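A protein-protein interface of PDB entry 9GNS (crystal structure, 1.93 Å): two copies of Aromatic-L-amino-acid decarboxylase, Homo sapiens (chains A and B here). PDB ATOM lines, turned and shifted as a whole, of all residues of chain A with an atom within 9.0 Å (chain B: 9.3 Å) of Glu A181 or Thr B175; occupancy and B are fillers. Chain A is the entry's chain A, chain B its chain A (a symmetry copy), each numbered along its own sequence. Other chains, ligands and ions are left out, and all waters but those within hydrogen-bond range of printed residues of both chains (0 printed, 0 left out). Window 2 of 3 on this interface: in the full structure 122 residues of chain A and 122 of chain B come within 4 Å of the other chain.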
ATOM      1  N   ILE A 164     -18.512 -31.945   6.158  1.00  0.00           N
ATOM      2  CA  ILE A 164     -19.367 -32.410   7.249  1.00  0.00           C
ATOM      3  C   ILE A 164     -19.957 -33.776   6.915  1.00  0.00           C
ATOM      4  O   ILE A 164     -19.981 -34.680   7.759  1.00  0.00           O
ATOM      5  CB  ILE A 164     -20.472 -31.381   7.561  1.00  0.00           C
ATOM      6  CG1 ILE A 164     -19.903 -30.184   8.332  1.00  0.00           C
ATOM      7  CG2 ILE A 164     -21.604 -32.023   8.368  1.00  0.00           C
ATOM      8  CD1 ILE A 164     -20.745 -28.928   8.172  1.00  0.00           C
ATOM      9  N   LEU A 167     -17.116 -36.461   7.092  1.00  0.00           N
ATOM     10  CA  LEU A 167     -16.694 -36.769   8.455  1.00  0.00           C
ATOM     11  C   LEU A 167     -17.780 -37.507   9.227  1.00  0.00           C
ATOM     12  O   LEU A 167     -17.468 -38.352  10.077  1.00  0.00           O
ATOM     13  CB  LEU A 167     -16.293 -35.484   9.185  1.00  0.00           C
ATOM     14  CG  LEU A 167     -15.082 -34.737   8.613  1.00  0.00           C
ATOM     15  CD1 LEU A 167     -14.801 -33.469   9.404  1.00  0.00           C
ATOM     16  CD2 LEU A 167     -13.860 -35.632   8.625  1.00  0.00           C
ATOM     17  N   LEU A 174     -20.883 -38.219  15.180  1.00  0.00           N
ATOM     18  CA  LEU A 174     -20.263 -36.902  15.245  1.00  0.00           C
ATOM     19  C   LEU A 174     -21.248 -35.813  14.829  1.00  0.00           C
ATOM     20  O   LEU A 174     -21.832 -35.873  13.743  1.00  0.00           O
ATOM     21  CB  LEU A 174     -19.031 -36.883  14.341  1.00  0.00           C
ATOM     22  CG  LEU A 174     -17.947 -35.830  14.533  1.00  0.00           C
ATOM     23  CD1 LEU A 174     -17.466 -35.818  15.975  1.00  0.00           C
ATOM     24  CD2 LEU A 174     -16.797 -36.112  13.575  1.00  0.00           C
ATOM     25  N   THR A 175     -21.422 -34.810  15.688  1.00  0.00           N
ATOM     26  CA  THR A 175     -22.361 -33.738  15.396  1.00  0.00           C
ATOM     27  C   THR A 175     -21.743 -32.717  14.445  1.00  0.00           C
ATOM     28  O   THR A 175     -20.520 -32.594  14.331  1.00  0.00           O
ATOM     29  CB  THR A 175     -22.790 -33.024  16.673  1.00  0.00           C
ATOM     30  OG1 THR A 175     -21.651 -32.375  17.252  1.00  0.00           O
ATOM     31  CG2 THR A 175     -23.351 -34.017  17.673  1.00  0.00           C
ATOM     32  N   GLN A 176     -22.614 -31.963  13.768  1.00  0.00           N
ATOM     33  CA  GLN A 176     -22.135 -30.881  12.914  1.00  0.00           C
ATOM     34  C   GLN A 176     -21.333 -29.862  13.718  1.00  0.00           C
ATOM     35  O   GLN A 176     -20.339 -29.317  13.227  1.00  0.00           O
ATOM     36  CB  GLN A 176     -23.306 -30.202  12.198  1.00  0.00           C
ATOM     37  CG  GLN A 176     -22.941 -28.873  11.540  1.00  0.00           C
ATOM     38  CD  GLN A 176     -23.837 -28.509  10.362  1.00  0.00           C
ATOM     39  OE1 GLN A 176     -24.298 -29.382   9.626  1.00  0.00           O
ATOM     40  NE2 GLN A 176     -24.061 -27.211  10.163  1.00  0.00           N
ATOM     41  N   ALA A 177     -21.734 -29.614  14.966  1.00  0.00           N
ATOM     42  CA  ALA A 177     -21.056 -28.601  15.768  1.00  0.00           C
ATOM     43  C   ALA A 177     -19.663 -29.057  16.188  1.00  0.00           C
ATOM     44  O   ALA A 177     -18.718 -28.260  16.178  1.00  0.00           O
ATOM     45  CB  ALA A 177     -21.903 -28.250  16.990  1.00  0.00           C
ATOM     46  N   ALA A 178     -19.514 -30.328  16.568  1.00  0.00           N
ATOM     47  CA  ALA A 178     -18.192 -30.835  16.921  1.00  0.00           C
ATOM     48  C   ALA A 178     -17.233 -30.735  15.740  1.00  0.00           C
ATOM     49  O   ALA A 178     -16.047 -30.436  15.913  1.00  0.00           O
ATOM     50  CB  ALA A 178     -18.289 -32.279  17.415  1.00  0.00           C
ATOM     51  N   ILE A 179     -17.737 -30.975  14.530  1.00  0.00           N
ATOM     52  CA  ILE A 179     -16.924 -30.811  13.330  1.00  0.00           C
ATOM     53  C   ILE A 179     -16.588 -29.343  13.113  1.00  0.00           C
ATOM     54  O   ILE A 179     -15.440 -28.993  12.811  1.00  0.00           O
ATOM     55  CB  ILE A 179     -17.665 -31.405  12.121  1.00  0.00           C
ATOM     56  CG1 ILE A 179     -17.767 -32.928  12.265  1.00  0.00           C
ATOM     57  CG2 ILE A 179     -17.000 -30.971  10.814  1.00  0.00           C
ATOM     58  CD1 ILE A 179     -18.836 -33.574  11.387  1.00  0.00           C
ATOM     59  N   MET A 180     -17.588 -28.468  13.266  1.00  0.00           N
ATOM     60  CA  MET A 180     -17.399 -27.028  13.096  1.00  0.00           C
ATOM     61  C   MET A 180     -16.230 -26.499  13.915  1.00  0.00           C
ATOM     62  O   MET A 180     -15.500 -25.607  13.468  1.00  0.00           O
ATOM     63  CB  MET A 180     -18.684 -26.296  13.490  1.00  0.00           C
ATOM     64  CG  MET A 180     -19.788 -26.376  12.464  1.00  0.00           C
ATOM     65  SD  MET A 180     -19.161 -26.059  10.814  1.00  0.00           S
ATOM     66  CE  MET A 180     -19.299 -24.273  10.766  1.00  0.00           C
ATOM     67  N   GLU A 181     -16.043 -27.037  15.121  1.00  0.00           N
ATOM     68  CA  GLU A 181     -14.966 -26.581  15.992  1.00  0.00           C
ATOM     69  C   GLU A 181     -13.595 -26.796  15.374  1.00  0.00           C
ATOM     70  O   GLU A 181     -12.653 -26.056  15.688  1.00  0.00           O
ATOM     71  CB  GLU A 181     -15.033 -27.310  17.330  1.00  0.00           C
ATOM     72  CG  GLU A 181     -14.870 -26.416  18.530  1.00  0.00           C
ATOM     73  CD  GLU A 181     -15.538 -26.999  19.744  1.00  0.00           C
ATOM     74  OE1 GLU A 181     -15.369 -28.211  19.990  1.00  0.00           O
ATOM     75  OE2 GLU A 181     -16.254 -26.254  20.440  1.00  0.00           O
ATOM     76  N   LYS A 182     -13.455 -27.802  14.513  1.00  0.00           N
ATOM     77  CA  LYS A 182     -12.136 -28.223  14.060  1.00  0.00           C
ATOM     78  C   LYS A 182     -11.818 -27.793  12.635  1.00  0.00           C
ATOM     79  O   LYS A 182     -10.644 -27.824  12.247  1.00  0.00           O
ATOM     80  CB  LYS A 182     -12.004 -29.748  14.166  1.00  0.00           C
ATOM     81  CG  LYS A 182     -12.098 -30.301  15.594  1.00  0.00           C
ATOM     82  CD  LYS A 182     -11.216 -29.526  16.576  1.00  0.00           C
ATOM     83  CE  LYS A 182     -11.161 -30.205  17.949  1.00  0.00           C
ATOM     84  NZ  LYS A 182     -10.418 -29.391  18.959  1.00  0.00           N
ATOM     85  N   LEU A 183     -12.818 -27.389  11.857  1.00  0.00           N
ATOM     86  CA  LEU A 183     -12.592 -27.015  10.465  1.00  0.00           C
ATOM     87  C   LEU A 183     -11.720 -25.770  10.368  1.00  0.00           C
ATOM     88  O   LEU A 183     -11.886 -24.816  11.131  1.00  0.00           O
ATOM     89  CB  LEU A 183     -13.924 -26.744   9.768  1.00  0.00           C
ATOM     90  CG  LEU A 183     -14.900 -27.902   9.554  1.00  0.00           C
ATOM     91  CD1 LEU A 183     -16.050 -27.451   8.655  1.00  0.00           C
ATOM     92  CD2 LEU A 183     -14.208 -29.128   8.984  1.00  0.00           C
ATOM     93  N   VAL A 184     -10.801 -25.768   9.404  1.00  0.00           N
ATOM     94  CA  VAL A 184      -9.985 -24.592   9.124  1.00  0.00           C
ATOM     95  C   VAL A 184      -9.886 -24.409   7.617  1.00  0.00           C
ATOM     96  O   VAL A 184      -9.726 -25.379   6.867  1.00  0.00           O
ATOM     97  CB  VAL A 184      -8.587 -24.683   9.785  1.00  0.00           C
ATOM     98  CG1 VAL A 184      -7.808 -25.901   9.283  1.00  0.00           C
ATOM     99  CG2 VAL A 184      -7.788 -23.395   9.531  1.00  0.00           C
ATOM    100  N   GLY A 202     -19.361 -18.307   7.271  1.00  0.00           N
ATOM    101  CA  GLY A 202     -19.424 -19.757   7.327  1.00  0.00           C
ATOM    102  C   GLY A 202     -19.169 -20.354   8.695  1.00  0.00           C
ATOM    103  O   GLY A 202     -19.393 -21.555   8.873  1.00  0.00           O
ATOM    104  N   GLY A 203     -18.703 -19.561   9.656  1.00  0.00           N
ATOM    105  CA  GLY A 203     -18.503 -20.074  11.003  1.00  0.00           C
ATOM    106  C   GLY A 203     -17.306 -20.987  11.162  1.00  0.00           C
ATOM    107  O   GLY A 203     -17.330 -21.884  12.011  1.00  0.00           O
ATOM    108  N   VAL A 204     -16.252 -20.783  10.370  1.00  0.00           N
ATOM    109  CA  VAL A 204     -15.060 -21.621  10.425  1.00  0.00           C
ATOM    110  C   VAL A 204     -13.830 -20.753  10.658  1.00  0.00           C
ATOM    111  O   VAL A 204     -13.816 -19.553  10.376  1.00  0.00           O
ATOM    112  CB  VAL A 204     -14.873 -22.468   9.145  1.00  0.00           C
ATOM    113  CG1 VAL A 204     -16.067 -23.385   8.940  1.00  0.00           C
ATOM    114  CG2 VAL A 204     -14.654 -21.568   7.915  1.00  0.00           C
ATOM    115  N   LYS A 205     -12.787 -21.388  11.189  1.00  0.00           N
ATOM    116  CA  LYS A 205     -11.501 -20.731  11.333  1.00  0.00           C
ATOM    117  C   LYS A 205     -10.860 -20.533   9.965  1.00  0.00           C
ATOM    118  O   LYS A 205     -11.056 -21.325   9.041  1.00  0.00           O
ATOM    119  CB  LYS A 205     -10.573 -21.560  12.222  1.00  0.00           C
ATOM    120  CG  LYS A 205     -11.081 -21.724  13.645  1.00  0.00           C
ATOM    121  CD  LYS A 205     -10.553 -23.012  14.270  1.00  0.00           C
ATOM    122  CE  LYS A 205     -10.900 -23.082  15.744  1.00  0.00           C
ATOM    123  NZ  LYS A 205     -12.375 -23.231  15.918  1.00  0.00           N
ATOM    124  N   ALA A 232      -2.503 -30.051  15.611  1.00  0.00           N
ATOM    125  CA  ALA A 232      -3.350 -29.428  16.623  1.00  0.00           C
ATOM    126  C   ALA A 232      -4.780 -29.961  16.628  1.00  0.00           C
ATOM    127  O   ALA A 232      -5.565 -29.558  17.494  1.00  0.00           O
ATOM    128  CB  ALA A 232      -3.374 -27.908  16.427  1.00  0.00           C
ATOM    129  N   GLY A 233      -5.143 -30.844  15.701  1.00  0.00           N
ATOM    130  CA  GLY A 233      -6.498 -31.357  15.633  1.00  0.00           C
ATOM    131  C   GLY A 233      -7.425 -30.584  14.724  1.00  0.00           C
ATOM    132  O   GLY A 233      -8.627 -30.878  14.688  1.00  0.00           O
ATOM    133  N   LEU A 234      -6.916 -29.600  13.995  1.00  0.00           N
ATOM    134  CA  LEU A 234      -7.732 -28.892  13.027  1.00  0.00           C
ATOM    135  C   LEU A 234      -7.902 -29.758  11.786  1.00  0.00           C
ATOM    136  O   LEU A 234      -7.066 -30.617  11.489  1.00  0.00           O
ATOM    137  CB  LEU A 234      -7.086 -27.552  12.676  1.00  0.00           C
ATOM    138  CG  LEU A 234      -7.069 -26.546  13.833  1.00  0.00           C
ATOM    139  CD1 LEU A 234      -6.531 -25.203  13.383  1.00  0.00           C
ATOM    140  CD2 LEU A 234      -8.467 -26.387  14.437  1.00  0.00           C
ATOM    141  N   ILE A 235      -9.002 -29.551  11.077  1.00  0.00           N
ATOM    142  CA  ILE A 235      -9.309 -30.292   9.862  1.00  0.00           C
ATOM    143  C   ILE A 235      -9.327 -29.323   8.689  1.00  0.00           C
ATOM    144  O   ILE A 235     -10.299 -28.583   8.496  1.00  0.00           O
ATOM    145  CB  ILE A 235     -10.634 -31.063   9.980  1.00  0.00           C
ATOM    146  CG1 ILE A 235     -10.572 -32.018  11.179  1.00  0.00           C
ATOM    147  CG2 ILE A 235     -10.940 -31.819   8.690  1.00  0.00           C
ATOM    148  CD1 ILE A 235     -11.858 -32.768  11.422  1.00  0.00           C
ATOM    149  N   VAL B 163     -26.074 -13.461  19.717  1.00  0.00           N
ATOM    150  CA  VAL B 163     -26.310 -14.435  20.783  1.00  0.00           C
ATOM    151  C   VAL B 163     -25.020 -15.156  21.165  1.00  0.00           C
ATOM    152  O   VAL B 163     -24.814 -15.484  22.342  1.00  0.00           O
ATOM    153  CB  VAL B 163     -27.435 -15.421  20.404  1.00  0.00           C
ATOM    154  CG1 VAL B 163     -27.001 -16.365  19.290  1.00  0.00           C
ATOM    155  CG2 VAL B 163     -27.867 -16.210  21.644  1.00  0.00           C
ATOM    156  N   ILE B 164     -24.116 -15.392  20.209  1.00  0.00           N
ATOM    157  CA  ILE B 164     -22.844 -16.016  20.567  1.00  0.00           C
ATOM    158  C   ILE B 164     -22.071 -15.126  21.536  1.00  0.00           C
ATOM    159  O   ILE B 164     -21.517 -15.606  22.532  1.00  0.00           O
ATOM    160  CB  ILE B 164     -22.012 -16.335  19.310  1.00  0.00           C
ATOM    161  CG1 ILE B 164     -22.568 -17.564  18.582  1.00  0.00           C
ATOM    162  CG2 ILE B 164     -20.542 -16.571  19.672  1.00  0.00           C
ATOM    163  CD1 ILE B 164     -22.197 -17.592  17.107  1.00  0.00           C
ATOM    164  N   HIS B 165     -22.024 -13.817  21.262  1.00  0.00           N
ATOM    165  CA  HIS B 165     -21.306 -12.908  22.154  1.00  0.00           C
ATOM    166  C   HIS B 165     -21.975 -12.819  23.520  1.00  0.00           C
ATOM    167  O   HIS B 165     -21.289 -12.761  24.546  1.00  0.00           O
ATOM    168  CB  HIS B 165     -21.187 -11.523  21.521  1.00  0.00           C
ATOM    169  CG  HIS B 165     -20.164 -11.449  20.430  1.00  0.00           C
ATOM    170  ND1 HIS B 165     -20.190 -10.486  19.444  1.00  0.00           N
ATOM    171  CD2 HIS B 165     -19.074 -12.215  20.178  1.00  0.00           C
ATOM    172  CE1 HIS B 165     -19.168 -10.667  18.625  1.00  0.00           C
ATOM    173  NE2 HIS B 165     -18.475 -11.709  19.050  1.00  0.00           N
ATOM    174  N   LEU B 167     -23.858 -15.190  25.016  1.00  0.00           N
ATOM    175  CA  LEU B 167     -23.681 -16.447  25.736  1.00  0.00           C
ATOM    176  C   LEU B 167     -22.241 -16.632  26.196  1.00  0.00           C
ATOM    177  O   LEU B 167     -22.001 -17.225  27.257  1.00  0.00           O
ATOM    178  CB  LEU B 167     -24.123 -17.622  24.861  1.00  0.00           C
ATOM    179  CG  LEU B 167     -25.609 -17.653  24.480  1.00  0.00           C
ATOM    180  CD1 LEU B 167     -25.919 -18.849  23.592  1.00  0.00           C
ATOM    181  CD2 LEU B 167     -26.469 -17.704  25.727  1.00  0.00           C
ATOM    182  N   GLN B 168     -21.276 -16.140  25.414  1.00  0.00           N
ATOM    183  CA  GLN B 168     -19.874 -16.210  25.815  1.00  0.00           C
ATOM    184  C   GLN B 168     -19.553 -15.199  26.905  1.00  0.00           C
ATOM    185  O   GLN B 168     -18.664 -15.440  27.731  1.00  0.00           O
ATOM    186  CB  GLN B 168     -18.969 -15.992  24.599  1.00  0.00           C
ATOM    187  CG  GLN B 168     -18.831 -17.231  23.727  1.00  0.00           C
ATOM    188  CD  GLN B 168     -17.970 -17.009  22.502  1.00  0.00           C
ATOM    189  OE1 GLN B 168     -17.849 -15.890  21.998  1.00  0.00           O
ATOM    190  NE2 GLN B 168     -17.347 -18.078  22.027  1.00  0.00           N
ATOM    191  N   SER B 171     -20.719 -17.159  29.848  1.00  0.00           N
ATOM    192  CA  SER B 171     -19.882 -18.336  30.094  1.00  0.00           C
ATOM    193  C   SER B 171     -18.619 -18.212  29.253  1.00  0.00           C
ATOM    194  O   SER B 171     -18.568 -18.700  28.115  1.00  0.00           O
ATOM    195  CB  SER B 171     -20.629 -19.630  29.771  1.00  0.00           C
ATOM    196  OG  SER B 171     -21.946 -19.629  30.305  1.00  0.00           O
ATOM    197  N   PRO B 172     -17.571 -17.572  29.784  1.00  0.00           N
ATOM    198  CA  PRO B 172     -16.372 -17.301  28.967  1.00  0.00           C
ATOM    199  C   PRO B 172     -15.690 -18.544  28.418  1.00  0.00           C
ATOM    200  O   PRO B 172     -14.983 -18.447  27.409  1.00  0.00           O
ATOM    201  CB  PRO B 172     -15.452 -16.556  29.943  1.00  0.00           C
ATOM    202  CG  PRO B 172     -16.395 -15.886  30.886  1.00  0.00           C
ATOM    203  CD  PRO B 172     -17.514 -16.877  31.082  1.00  0.00           C
ATOM    204  N   GLU B 173     -15.863 -19.704  29.049  1.00  0.00           N
ATOM    205  CA  GLU B 173     -15.267 -20.944  28.569  1.00  0.00           C
ATOM    206  C   GLU B 173     -16.003 -21.544  27.375  1.00  0.00           C
ATOM    207  O   GLU B 173     -15.484 -22.477  26.754  1.00  0.00           O
ATOM    208  CB  GLU B 173     -15.222 -21.964  29.711  1.00  0.00           C
ATOM    209  CG  GLU B 173     -16.420 -22.913  29.749  1.00  0.00           C
ATOM    210  CD  GLU B 173     -17.639 -22.308  30.436  1.00  0.00           C
ATOM    211  OE1 GLU B 173     -17.589 -21.115  30.813  1.00  0.00           O
ATOM    212  OE2 GLU B 173     -18.651 -23.028  30.591  1.00  0.00           O
ATOM    213  N   LEU B 174     -17.180 -21.024  27.033  1.00  0.00           N
ATOM    214  CA  LEU B 174     -18.062 -21.661  26.062  1.00  0.00           C
ATOM    215  C   LEU B 174     -17.607 -21.365  24.636  1.00  0.00           C
ATOM    216  O   LEU B 174     -17.445 -20.201  24.254  1.00  0.00           O
ATOM    217  CB  LEU B 174     -19.491 -21.166  26.282  1.00  0.00           C
ATOM    218  CG  LEU B 174     -20.675 -21.957  25.741  1.00  0.00           C
ATOM    219  CD1 LEU B 174     -20.606 -23.402  26.208  1.00  0.00           C
ATOM    220  CD2 LEU B 174     -21.970 -21.296  26.196  1.00  0.00           C
ATOM    221  N   THR B 175     -17.414 -22.418  23.844  1.00  0.00           N
ATOM    222  CA  THR B 175     -16.953 -22.242  22.475  1.00  0.00           C
ATOM    223  C   THR B 175     -18.110 -21.860  21.556  1.00  0.00           C
ATOM    224  O   THR B 175     -19.282 -22.114  21.848  1.00  0.00           O
ATOM    225  CB  THR B 175     -16.309 -23.520  21.947  1.00  0.00           C
ATOM    226  OG1 THR B 175     -17.301 -24.552  21.878  1.00  0.00           O
ATOM    227  CG2 THR B 175     -15.194 -23.972  22.871  1.00  0.00           C
ATOM    228  N   GLN B 176     -17.762 -21.250  20.420  1.00  0.00           N
ATOM    229  CA  GLN B 176     -18.775 -20.938  19.417  1.00  0.00           C
ATOM    230  C   GLN B 176     -19.482 -22.202  18.940  1.00  0.00           C
ATOM    231  O   GLN B 176     -20.692 -22.187  18.685  1.00  0.00           O
ATOM    232  CB  GLN B 176     -18.150 -20.189  18.235  1.00  0.00           C
ATOM    233  CG  GLN B 176     -19.058 -20.104  17.010  1.00  0.00           C
ATOM    234  CD  GLN B 176     -18.761 -18.909  16.113  1.00  0.00           C
ATOM    235  OE1 GLN B 176     -18.374 -17.842  16.589  1.00  0.00           O
ATOM    236  NE2 GLN B 176     -18.969 -19.078  14.808  1.00  0.00           N
ATOM    237  N   ALA B 177     -18.752 -23.314  18.841  1.00  0.00           N
ATOM    238  CA  ALA B 177     -19.346 -24.542  18.325  1.00  0.00           C
ATOM    239  C   ALA B 177     -20.332 -25.147  19.319  1.00  0.00           C
ATOM    240  O   ALA B 177     -21.395 -25.637  18.920  1.00  0.00           O
ATOM    241  CB  ALA B 177     -18.250 -25.544  17.971  1.00  0.00           C
ATOM    242  N   ALA B 178     -19.999 -25.132  20.612  1.00  0.00           N
ATOM    243  CA  ALA B 178     -20.932 -25.643  21.612  1.00  0.00           C
ATOM    244  C   ALA B 178     -22.233 -24.848  21.603  1.00  0.00           C
ATOM    245  O   ALA B 178     -23.318 -25.412  21.782  1.00  0.00           O
ATOM    246  CB  ALA B 178     -20.292 -25.613  23.000  1.00  0.00           C
ATOM    247  N   ILE B 179     -22.141 -23.536  21.386  1.00  0.00           N
ATOM    248  CA  ILE B 179     -23.334 -22.708  21.264  1.00  0.00           C
ATOM    249  C   ILE B 179     -24.097 -23.061  19.998  1.00  0.00           C
ATOM    250  O   ILE B 179     -25.327 -23.197  20.015  1.00  0.00           O
ATOM    251  CB  ILE B 179     -22.934 -21.223  21.288  1.00  0.00           C
ATOM    252  CG1 ILE B 179     -22.393 -20.849  22.673  1.00  0.00           C
ATOM    253  CG2 ILE B 179     -24.103 -20.343  20.845  1.00  0.00           C
ATOM    254  CD1 ILE B 179     -21.569 -19.564  22.701  1.00  0.00           C
ATOM    255  N   MET B 180     -23.375 -23.212  18.882  1.00  0.00           N
ATOM    256  CA  MET B 180     -23.983 -23.561  17.598  1.00  0.00           C
ATOM    257  C   MET B 180     -24.886 -24.781  17.700  1.00  0.00           C
ATOM    258  O   MET B 180     -25.934 -24.845  17.046  1.00  0.00           O
ATOM    259  CB  MET B 180     -22.882 -23.812  16.566  1.00  0.00           C
ATOM    260  CG  MET B 180     -22.227 -22.560  16.033  1.00  0.00           C
ATOM    261  SD  MET B 180     -23.451 -21.321  15.609  1.00  0.00           S
ATOM    262  CE  MET B 180     -23.814 -21.802  13.922  1.00  0.00           C
ATOM    263  N   GLU B 181     -24.492 -25.761  18.513  1.00  0.00           N
ATOM    264  CA  GLU B 181     -25.275 -26.982  18.661  1.00  0.00           C
ATOM    265  C   GLU B 181     -26.668 -26.711  19.204  1.00  0.00           C
ATOM    266  O   GLU B 181     -27.599 -27.477  18.926  1.00  0.00           O
ATOM    267  CB  GLU B 181     -24.555 -27.955  19.589  1.00  0.00           C
ATOM    268  CG  GLU B 181     -24.517 -29.374  19.087  1.00  0.00           C
ATOM    269  CD  GLU B 181     -23.339 -30.123  19.645  1.00  0.00           C
ATOM    270  OE1 GLU B 181     -23.087 -30.009  20.863  1.00  0.00           O
ATOM    271  OE2 GLU B 181     -22.648 -30.803  18.863  1.00  0.00           O
ATOM    272  N   LYS B 182     -26.831 -25.646  19.987  1.00  0.00           N
ATOM    273  CA  LYS B 182     -28.064 -25.446  20.734  1.00  0.00           C
ATOM    274  C   LYS B 182     -28.963 -24.366  20.149  1.00  0.00           C
ATOM    275  O   LYS B 182     -30.145 -24.310  20.506  1.00  0.00           O
ATOM    276  CB  LYS B 182     -27.745 -25.098  22.195  1.00  0.00           C
ATOM    277  CG  LYS B 182     -27.016 -26.202  22.972  1.00  0.00           C
ATOM    278  CD  LYS B 182     -27.670 -27.573  22.784  1.00  0.00           C
ATOM    279  CE  LYS B 182     -27.061 -28.626  23.716  1.00  0.00           C
ATOM    280  NZ  LYS B 182     -27.589 -30.000  23.449  1.00  0.00           N
ATOM    281  N   LEU B 183     -28.442 -23.521  19.265  1.00  0.00           N
ATOM    282  CA  LEU B 183     -29.229 -22.428  18.704  1.00  0.00           C
ATOM    283  C   LEU B 183     -30.374 -22.960  17.854  1.00  0.00           C
ATOM    284  O   LEU B 183     -30.209 -23.913  17.089  1.00  0.00           O
ATOM    285  CB  LEU B 183     -28.347 -21.528  17.842  1.00  0.00           C
ATOM    286  CG  LEU B 183     -27.240 -20.711  18.511  1.00  0.00           C
ATOM    287  CD1 LEU B 183     -26.638 -19.731  17.506  1.00  0.00           C
ATOM    288  CD2 LEU B 183     -27.739 -19.987  19.750  1.00  0.00           C
ATOM    289  N   ILE B 235     -31.578 -23.130  22.404  1.00  0.00           N
ATOM    290  CA  ILE B 235     -31.531 -21.709  22.712  1.00  0.00           C
ATOM    291  C   ILE B 235     -32.180 -20.939  21.570  1.00  0.00           C
ATOM    292  O   ILE B 235     -31.567 -20.741  20.516  1.00  0.00           O
ATOM    293  CB  ILE B 235     -30.096 -21.226  22.977  1.00  0.00           C
ATOM    294  CG1 ILE B 235     -29.481 -22.036  24.127  1.00  0.00           C
ATOM    295  CG2 ILE B 235     -30.074 -19.732  23.284  1.00  0.00           C
ATOM    296  CD1 ILE B 235     -28.042 -21.681  24.414  1.00  0.00           C
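The side-chain carboxylate (OE2) of Glu B181 lies within hydrogen-bond range of the side-chain hydroxyl (OG1) of Thr A175 (2.5 Å).
OG1 of Thr B175 lies within hydrogen-bond range of OE2 of Glu A181 (2.5 Å).
The backbone carbonyl oxygen of Glu A181 lies within hydrogen-bond range of the side-chain amino group of Lys A205.
The backbone NH (N) of Ala A178 sits at hydrogen-bond distance from the side-chain hydroxyl (OG1) of Thr A175, at 3.0 Å.
N of Ala B178 is in hydrogen-bond range of OG1 of Thr B175 (3.0 Å).
O of Ala A177 touches CB of Ala B177 (3.3 Å).
Glu B181 touches Ala A177.
Glu B181 touches Ala A178.
CB of Ala B177 touches OE2 of Glu A181, at 3.3 Å.
N of Ala B178 touches OE2 of Glu A181 (3.9 Å).
Gly A203 touches Gln B176.
Of the printed residues of chain B, Thr A175 touches Glu B181.
Glu A181 touches just these residues of chain B: Thr B175, Ala B177 and Ala B178.
Printed residues of chain B within 4 Å of Gly A203: Gln B176.
Of the printed residues of chain A, Gln B176 touches Gly A203.
The nearest printed residue of chain B that does not touch Thr A175 is Ala B177 (6.9 Å).
Of the 19 printed residues of chain B, 5 touch a printed residue of chain A.
Hydrophobic or aromatic side chains of chain B that line the printed part of chain A: Ala B177.
Of the 21 printed residues of chain A, 5 touch a printed residue of chain B.
Hydrophobic or aromatic side chains of chain A that line the printed part of chain B: Ala A177.
Among the printed residues, no Asp or Glu carboxylate lies within 4 Å of a Lys or Arg side-chain nitrogen of the other chain.
Thr A175 touches Glu B181, and with the chains exchanged Glu A181 touches Thr B175.
Ala A177 touches its own counterpart, Ala B177.
Ala A177 touches Glu B181, and with the chains exchanged Glu A181 touches Ala B177.
Ala A178 touches Glu B181, and with the chains exchanged Glu A181 touches Ala B178.
Positions printed for both chains: 164, 167, 174, 175, 176, 177, 178, 179, 180, 181, 182, 183 and 235.
Of the 8 pairs that touch across the chains among the printed residues, 7 have their exchanged pair printed and touching as well.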
